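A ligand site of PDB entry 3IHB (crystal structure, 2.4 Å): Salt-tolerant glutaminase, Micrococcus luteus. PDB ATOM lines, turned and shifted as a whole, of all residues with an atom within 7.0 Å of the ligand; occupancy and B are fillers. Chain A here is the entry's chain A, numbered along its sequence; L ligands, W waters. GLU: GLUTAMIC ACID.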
ATOM      1  N   TYR A  27      -6.174  18.295 -14.184  1.00  0.00           N
ATOM      2  CA  TYR A  27      -5.901  19.696 -14.484  1.00  0.00           C
ATOM      3  C   TYR A  27      -5.866  20.179 -15.942  1.00  0.00           C
ATOM      4  O   TYR A  27      -5.385  21.274 -16.235  1.00  0.00           O
ATOM      5  CB  TYR A  27      -4.616  20.130 -13.769  1.00  0.00           C
ATOM      6  CG  TYR A  27      -3.349  19.409 -14.166  1.00  0.00           C
ATOM      7  CD1 TYR A  27      -2.561  19.874 -15.216  1.00  0.00           C
ATOM      8  CD2 TYR A  27      -2.910  18.286 -13.463  1.00  0.00           C
ATOM      9  CE1 TYR A  27      -1.357  19.238 -15.551  1.00  0.00           C
ATOM     10  CE2 TYR A  27      -1.714  17.648 -13.783  1.00  0.00           C
ATOM     11  CZ  TYR A  27      -0.937  18.132 -14.828  1.00  0.00           C
ATOM     12  OH  TYR A  27       0.250  17.530 -15.146  1.00  0.00           O
ATOM     13  N   ILE A  28      -6.413  19.376 -16.848  1.00  0.00           N
ATOM     14  CA  ILE A  28      -6.477  19.715 -18.275  1.00  0.00           C
ATOM     15  C   ILE A  28      -7.670  18.930 -18.814  1.00  0.00           C
ATOM     16  O   ILE A  28      -7.567  17.739 -19.103  1.00  0.00           O
ATOM     17  CB  ILE A  28      -5.188  19.290 -19.030  1.00  0.00           C
ATOM     18  CG1 ILE A  28      -4.004  20.125 -18.519  1.00  0.00           C
ATOM     19  CG2 ILE A  28      -5.360  19.477 -20.530  1.00  0.00           C
ATOM     20  CD1 ILE A  28      -2.657  19.700 -19.084  1.00  0.00           C
ATOM     21  N   LEU A  31      -7.580  15.813 -21.176  1.00  0.00           N
ATOM     22  CA  LEU A  31      -7.008  14.584 -20.634  1.00  0.00           C
ATOM     23  C   LEU A  31      -7.903  13.943 -19.569  1.00  0.00           C
ATOM     24  O   LEU A  31      -7.903  12.723 -19.413  1.00  0.00           O
ATOM     25  CB  LEU A  31      -5.626  14.836 -20.047  1.00  0.00           C
ATOM     26  CG  LEU A  31      -4.481  15.158 -21.005  1.00  0.00           C
ATOM     27  CD1 LEU A  31      -3.219  15.465 -20.206  1.00  0.00           C
ATOM     28  CD2 LEU A  31      -4.262  13.986 -21.959  1.00  0.00           C
ATOM     29  N   ILE A  62       2.691  12.849 -25.506  1.00  0.00           N
ATOM     30  CA  ILE A  62       3.818  12.318 -24.752  1.00  0.00           C
ATOM     31  C   ILE A  62       4.137  13.077 -23.466  1.00  0.00           C
ATOM     32  O   ILE A  62       4.724  12.518 -22.543  1.00  0.00           O
ATOM     33  CB  ILE A  62       5.072  12.274 -25.654  1.00  0.00           C
ATOM     34  CG1 ILE A  62       6.195  11.512 -24.959  1.00  0.00           C
ATOM     35  CG2 ILE A  62       5.476  13.665 -26.051  1.00  0.00           C
ATOM     36  CD1 ILE A  62       7.399  11.227 -25.853  1.00  0.00           C
ATOM     37  N   GLN A  63       3.728  14.335 -23.396  1.00  0.00           N
ATOM     38  CA  GLN A  63       3.962  15.140 -22.207  1.00  0.00           C
ATOM     39  C   GLN A  63       5.387  15.003 -21.650  1.00  0.00           C
ATOM     40  O   GLN A  63       6.350  15.055 -22.412  1.00  0.00           O
ATOM     41  CB  GLN A  63       2.930  14.765 -21.145  1.00  0.00           C
ATOM     42  CG  GLN A  63       1.470  14.970 -21.588  1.00  0.00           C
ATOM     43  CD  GLN A  63       1.134  16.414 -21.949  1.00  0.00           C
ATOM     44  OE1 GLN A  63       1.582  17.358 -21.303  1.00  0.00           O
ATOM     45  NE2 GLN A  63       0.313  16.603 -22.987  1.00  0.00           N
ATOM     46  N   SER A  64       5.516  14.810 -20.340  1.00  0.00           N
ATOM     47  CA  SER A  64       6.820  14.707 -19.677  1.00  0.00           C
ATOM     48  C   SER A  64       7.795  13.753 -20.329  1.00  0.00           C
ATOM     49  O   SER A  64       9.002  13.993 -20.298  1.00  0.00           O
ATOM     50  CB  SER A  64       6.674  14.318 -18.206  1.00  0.00           C
ATOM     51  OG  SER A  64       6.548  15.464 -17.366  1.00  0.00           O
ATOM     52  N   ALA A  65       7.288  12.661 -20.901  1.00  0.00           N
ATOM     53  CA  ALA A  65       8.174  11.707 -21.535  1.00  0.00           C
ATOM     54  C   ALA A  65       8.946  12.338 -22.701  1.00  0.00           C
ATOM     55  O   ALA A  65       9.815  11.695 -23.265  1.00  0.00           O
ATOM     56  CB  ALA A  65       7.371  10.505 -22.022  1.00  0.00           C
ATOM     57  N   LYS A  67      10.641  15.186 -22.360  1.00  0.00           N
ATOM     58  CA  LYS A  67      11.774  15.838 -21.699  1.00  0.00           C
ATOM     59  C   LYS A  67      13.166  15.253 -21.963  1.00  0.00           C
ATOM     60  O   LYS A  67      14.121  15.992 -22.166  1.00  0.00           O
ATOM     61  CB  LYS A  67      11.500  15.912 -20.197  1.00  0.00           C
ATOM     62  CG  LYS A  67      10.466  16.967 -19.851  1.00  0.00           C
ATOM     63  CD  LYS A  67      10.065  16.904 -18.403  1.00  0.00           C
ATOM     64  CE  LYS A  67       9.084  18.003 -18.079  1.00  0.00           C
ATOM     65  NZ  LYS A  67       8.456  17.785 -16.764  1.00  0.00           N
ATOM     66  N   GLU A  94       8.596  17.771  -7.986  1.00  0.00           N
ATOM     67  CA  GLU A  94       8.145  18.755  -8.955  1.00  0.00           C
ATOM     68  C   GLU A  94       7.781  20.052  -8.235  1.00  0.00           C
ATOM     69  O   GLU A  94       7.766  21.118  -8.846  1.00  0.00           O
ATOM     70  CB  GLU A  94       6.954  18.217  -9.759  1.00  0.00           C
ATOM     71  CG  GLU A  94       6.334  19.205 -10.771  1.00  0.00           C
ATOM     72  CD  GLU A  94       7.362  19.865 -11.694  1.00  0.00           C
ATOM     73  OE1 GLU A  94       7.317  21.115 -11.795  1.00  0.00           O
ATOM     74  OE2 GLU A  94       8.196  19.171 -12.314  1.00  0.00           O
ATOM     75  N   MET A 112      14.209  16.758 -15.824  1.00  0.00           N
ATOM     76  CA  MET A 112      12.957  16.004 -15.757  1.00  0.00           C
ATOM     77  C   MET A 112      11.826  16.812 -15.164  1.00  0.00           C
ATOM     78  O   MET A 112      10.656  16.505 -15.387  1.00  0.00           O
ATOM     79  CB  MET A 112      13.147  14.711 -14.941  1.00  0.00           C
ATOM     80  CG  MET A 112      14.150  13.739 -15.541  1.00  0.00           C
ATOM     81  SD  MET A 112      13.870  13.486 -17.302  1.00  0.00           S
ATOM     82  CE  MET A 112      12.974  12.033 -17.248  1.00  0.00           C
ATOM     83  N   ASN A 114       9.596  20.313 -14.681  1.00  0.00           N
ATOM     84  CA  ASN A 114       9.105  21.365 -15.571  1.00  0.00           C
ATOM     85  C   ASN A 114      10.063  22.551 -15.689  1.00  0.00           C
ATOM     86  O   ASN A 114      10.416  22.955 -16.799  1.00  0.00           O
ATOM     87  CB  ASN A 114       7.730  21.861 -15.102  1.00  0.00           C
ATOM     88  CG  ASN A 114       6.640  20.812 -15.256  1.00  0.00           C
ATOM     89  OD1 ASN A 114       6.921  19.647 -15.578  1.00  0.00           O
ATOM     90  ND2 ASN A 114       5.397  21.208 -15.021  1.00  0.00           N
ATOM     91  N   GLU A 160      -4.384  23.184 -22.802  1.00  0.00           N
ATOM     92  CA  GLU A 160      -3.418  23.419 -21.738  1.00  0.00           C
ATOM     93  C   GLU A 160      -2.935  24.868 -21.695  1.00  0.00           C
ATOM     94  O   GLU A 160      -2.689  25.402 -20.624  1.00  0.00           O
ATOM     95  CB  GLU A 160      -2.220  22.467 -21.876  1.00  0.00           C
ATOM     96  CG  GLU A 160      -1.026  22.865 -21.024  1.00  0.00           C
ATOM     97  CD  GLU A 160      -0.045  21.732 -20.749  1.00  0.00           C
ATOM     98  OE1 GLU A 160       0.044  20.782 -21.559  1.00  0.00           O
ATOM     99  OE2 GLU A 160       0.653  21.801 -19.714  1.00  0.00           O
ATOM    100  N   ARG A 166       0.825  27.925 -13.838  1.00  0.00           N
ATOM    101  CA  ARG A 166       1.926  27.339 -13.082  1.00  0.00           C
ATOM    102  C   ARG A 166       3.226  27.374 -13.890  1.00  0.00           C
ATOM    103  O   ARG A 166       4.232  27.866 -13.401  1.00  0.00           O
ATOM    104  CB  ARG A 166       1.603  25.893 -12.645  1.00  0.00           C
ATOM    105  CG  ARG A 166       2.715  25.266 -11.805  1.00  0.00           C
ATOM    106  CD  ARG A 166       2.287  23.950 -11.153  1.00  0.00           C
ATOM    107  NE  ARG A 166       3.326  23.401 -10.264  1.00  0.00           N
ATOM    108  CZ  ARG A 166       4.452  22.826 -10.677  1.00  0.00           C
ATOM    109  NH1 ARG A 166       4.712  22.680 -11.960  1.00  0.00           N
ATOM    110  NH2 ARG A 166       5.337  22.386  -9.783  1.00  0.00           N
ATOM    111  N   ASN A 167       3.208  26.853 -15.115  1.00  0.00           N
ATOM    112  CA  ASN A 167       4.425  26.872 -15.932  1.00  0.00           C
ATOM    113  C   ASN A 167       4.858  28.299 -16.306  1.00  0.00           C
ATOM    114  O   ASN A 167       6.040  28.553 -16.512  1.00  0.00           O
ATOM    115  CB  ASN A 167       4.250  26.025 -17.203  1.00  0.00           C
ATOM    116  CG  ASN A 167       4.357  24.537 -16.928  1.00  0.00           C
ATOM    117  OD1 ASN A 167       5.187  24.094 -16.139  1.00  0.00           O
ATOM    118  ND2 ASN A 167       3.530  23.748 -17.609  1.00  0.00           N
ATOM    119  N   TYR A 191       7.126  24.788 -25.062  1.00  0.00           N
ATOM    120  CA  TYR A 191       7.153  23.585 -24.224  1.00  0.00           C
ATOM    121  C   TYR A 191       5.802  22.876 -24.196  1.00  0.00           C
ATOM    122  O   TYR A 191       5.743  21.641 -24.215  1.00  0.00           O
ATOM    123  CB  TYR A 191       7.589  23.961 -22.794  1.00  0.00           C
ATOM    124  CG  TYR A 191       7.324  22.895 -21.735  1.00  0.00           C
ATOM    125  CD1 TYR A 191       8.108  21.737 -21.678  1.00  0.00           C
ATOM    126  CD2 TYR A 191       6.297  23.057 -20.802  1.00  0.00           C
ATOM    127  CE1 TYR A 191       7.862  20.761 -20.711  1.00  0.00           C
ATOM    128  CE2 TYR A 191       6.064  22.081 -19.829  1.00  0.00           C
ATOM    129  CZ  TYR A 191       6.833  20.946 -19.788  1.00  0.00           C
ATOM    130  OH  TYR A 191       6.576  19.987 -18.831  1.00  0.00           O
ATOM    131  N   VAL A 192       4.712  23.655 -24.158  1.00  0.00           N
ATOM    132  CA  VAL A 192       3.376  23.060 -24.139  1.00  0.00           C
ATOM    133  C   VAL A 192       3.063  22.366 -25.463  1.00  0.00           C
ATOM    134  O   VAL A 192       2.345  21.356 -25.503  1.00  0.00           O
ATOM    135  CB  VAL A 192       2.292  24.127 -23.864  1.00  0.00           C
ATOM    136  CG1 VAL A 192       0.927  23.474 -23.779  1.00  0.00           C
ATOM    137  CG2 VAL A 192       2.595  24.854 -22.566  1.00  0.00           C
ATOM    138  N   CYS A 195       5.007  19.160 -25.406  1.00  0.00           N
ATOM    139  CA  CYS A 195       4.324  18.123 -24.627  1.00  0.00           C
ATOM    140  C   CYS A 195       3.122  17.539 -25.352  1.00  0.00           C
ATOM    141  O   CYS A 195       2.637  16.467 -24.991  1.00  0.00           O
ATOM    142  CB  CYS A 195       3.853  18.697 -23.283  1.00  0.00           C
ATOM    143  SG  CYS A 195       5.177  19.076 -22.118  1.00  0.00           S
ATOM    144  N   ALA A 196       2.654  18.253 -26.374  1.00  0.00           N
ATOM    145  CA  ALA A 196       1.487  17.823 -27.144  1.00  0.00           C
ATOM    146  C   ALA A 196       1.794  16.935 -28.343  1.00  0.00           C
ATOM    147  O   ALA A 196       0.878  16.540 -29.072  1.00  0.00           O
ATOM    148  CB  ALA A 196       0.692  19.043 -27.582  1.00  0.00           C
ATOM    149  N   TYR A 243      11.478  11.362  -9.418  1.00  0.00           N
ATOM    150  CA  TYR A 243      11.565  12.375  -8.382  1.00  0.00           C
ATOM    151  C   TYR A 243      12.114  11.897  -7.026  1.00  0.00           C
ATOM    152  O   TYR A 243      13.184  11.297  -6.975  1.00  0.00           O
ATOM    153  CB  TYR A 243      10.177  13.018  -8.198  1.00  0.00           C
ATOM    154  CG  TYR A 243       9.548  13.464  -9.510  1.00  0.00           C
ATOM    155  CD1 TYR A 243       8.721  12.603 -10.238  1.00  0.00           C
ATOM    156  CD2 TYR A 243       9.822  14.731 -10.040  1.00  0.00           C
ATOM    157  CE1 TYR A 243       8.182  12.988 -11.467  1.00  0.00           C
ATOM    158  CE2 TYR A 243       9.288  15.124 -11.292  1.00  0.00           C
ATOM    159  CZ  TYR A 243       8.472  14.248 -11.997  1.00  0.00           C
ATOM    160  OH  TYR A 243       7.931  14.601 -13.206  1.00  0.00           O
ATOM    161  N   LYS A 258      10.490   7.407 -17.400  1.00  0.00           N
ATOM    162  CA  LYS A 258       9.762   8.647 -17.186  1.00  0.00           C
ATOM    163  C   LYS A 258       8.333   8.466 -17.639  1.00  0.00           C
ATOM    164  O   LYS A 258       8.074   7.969 -18.743  1.00  0.00           O
ATOM    165  CB  LYS A 258      10.373   9.816 -17.959  1.00  0.00           C
ATOM    166  CG  LYS A 258       9.786  11.176 -17.554  1.00  0.00           C
ATOM    167  CD  LYS A 258      10.090  11.451 -16.061  1.00  0.00           C
ATOM    168  CE  LYS A 258       9.427  12.726 -15.533  1.00  0.00           C
ATOM    169  NZ  LYS A 258       7.952  12.508 -15.392  1.00  0.00           N
ATOM    170  N   SER A 259       7.407   8.881 -16.797  1.00  0.00           N
ATOM    171  CA  SER A 259       5.990   8.790 -17.105  1.00  0.00           C
ATOM    172  C   SER A 259       5.509  10.163 -17.571  1.00  0.00           C
ATOM    173  O   SER A 259       6.170  11.170 -17.350  1.00  0.00           O
ATOM    174  CB  SER A 259       5.217   8.339 -15.872  1.00  0.00           C
ATOM    175  OG  SER A 259       3.819   8.444 -16.074  1.00  0.00           O
ATOM    176  N   GLY A 260       4.346  10.186 -18.214  1.00  0.00           N
ATOM    177  CA  GLY A 260       3.727  11.413 -18.682  1.00  0.00           C
ATOM    178  C   GLY A 260       2.280  11.398 -18.228  1.00  0.00           C
ATOM    179  O   GLY A 260       1.651  10.335 -18.256  1.00  0.00           O
ATOM    180  N   VAL A 261       1.744  12.542 -17.822  1.00  0.00           N
ATOM    181  CA  VAL A 261       0.369  12.615 -17.320  1.00  0.00           C
ATOM    182  C   VAL A 261      -0.768  12.198 -18.265  1.00  0.00           C
ATOM    183  O   VAL A 261      -1.943  12.257 -17.883  1.00  0.00           O
ATOM    184  CB  VAL A 261       0.049  14.025 -16.768  1.00  0.00           C
ATOM    185  CG1 VAL A 261       1.063  14.376 -15.715  1.00  0.00           C
ATOM    186  CG2 VAL A 261       0.054  15.049 -17.882  1.00  0.00           C
ATOM    187  N   ALA A 262      -0.434  11.790 -19.485  1.00  0.00           N
ATOM    188  CA  ALA A 262      -1.447  11.353 -20.439  1.00  0.00           C
ATOM    189  C   ALA A 262      -1.574   9.826 -20.384  1.00  0.00           C
ATOM    190  O   ALA A 262      -2.380   9.217 -21.100  1.00  0.00           O
ATOM    191  CB  ALA A 262      -1.085  11.798 -21.863  1.00  0.00           C
ATOM    192  N   GLY A 264       1.308   7.737 -20.648  1.00  0.00           N
ATOM    193  CA  GLY A 264       2.478   7.071 -21.206  1.00  0.00           C
ATOM    194  C   GLY A 264       3.712   6.954 -20.323  1.00  0.00           C
ATOM    195  O   GLY A 264       4.006   7.836 -19.526  1.00  0.00           O
ATOM    196  N   GLY A 286       1.023  11.039  -9.445  1.00  0.00           N
ATOM    197  CA  GLY A 286       1.064  11.510 -10.824  1.00  0.00           C
ATOM    198  C   GLY A 286       1.552  10.604 -11.942  1.00  0.00           C
ATOM    199  O   GLY A 286       1.523  11.021 -13.102  1.00  0.00           O
HETATM  200  N   GLU L   1       2.410  19.148 -19.693  1.00  0.00           N
HETATM  201  CA  GLU L   1       2.471  19.050 -18.223  1.00  0.00           C
HETATM  202  C   GLU L   1       2.914  20.351 -17.586  1.00  0.00           C
HETATM  203  O   GLU L   1       2.717  20.546 -16.405  1.00  0.00           O
HETATM  204  CB  GLU L   1       3.426  17.941 -17.764  1.00  0.00           C
HETATM  205  CG  GLU L   1       2.800  16.573 -17.748  1.00  0.00           C
HETATM  206  CD  GLU L   1       3.703  15.483 -17.162  1.00  0.00           C
HETATM  207  OE1 GLU L   1       4.200  15.646 -16.018  1.00  0.00           O
HETATM  208  OE2 GLU L   1       3.907  14.460 -17.830  1.00  0.00           O
HETATM  209  O   HOH W   1       4.787  17.247 -13.664  1.00  0.00           O
HETATM  210  O   HOH W   2       1.887  21.910 -13.809  1.00  0.00           O
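OE1 of the ligand sits at hydrogen-bond distance from OG of Ser 64.
The backbone NH (N) of Val 261 sits at hydrogen-bond distance from an oxygen (OE2) of the ligand, at 2.9 Å.
A nitrogen (N) of the ligand lies within salt-bridge range of the side-chain carboxylate (OE2) of Glu 160.
N of the ligand sits at hydrogen-bond distance from SG of Cys 195 (3.7 Å).
N of Ser 64 lies close to OE2 of the ligand (3.0 Å).
An oxygen (O) of the ligand lies within hydrogen-bond range of the side-chain amide nitrogen of Asn 114 (3.1 Å).
A nitrogen (N) of the ligand sits at hydrogen-bond distance from the side-chain amide oxygen of Gln 63, at 2.5 Å.
Tyr 27 touches the ligand.
Asn 167 touches the ligand.
OH of Tyr 191 touches C of the ligand, 3.9 Å away.
Gly 260 touches the ligand (CA to OE2, 3.2 Å).
Hydrophobic or aromatic side chains within 4 Å of the ligand: Val 261.
Of the 26 residues printed, 10 come within 4 Å of the ligand.
Water W2 bridges an oxygen (O) of the ligand and the guanidinium group of Arg 166.
The side-chain amide nitrogen of Asn 114 is in hydrogen-bond range of the side-chain amide oxygen of Asn 167 (3.1 Å).
O of Tyr 191 lies within hydrogen-bond range of SG of Cys 195, at 3.4 Å.
The side-chain hydroxyl of Tyr 191 is in hydrogen-bond range of the side-chain amide oxygen of Asn 114 (3.3 Å).
The backbone NH (N) of Gln 63 lies within hydrogen-bond range of the backbone carbonyl oxygen (O) of Cys 195, at 2.9 Å.
OD1 of Asn 114 sits at hydrogen-bond distance from NZ of Lys 67, at 2.7 Å.
OG of Ser 64 lies within hydrogen-bond range of NZ of Lys 67.
The side-chain amide nitrogen (ND2) of Asn 114 sits close to the guanidinium group (NH1) of Arg 166.
The side-chain carboxylate of Glu 94 lies within hydrogen-bond range of the backbone NH of Asn 114.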
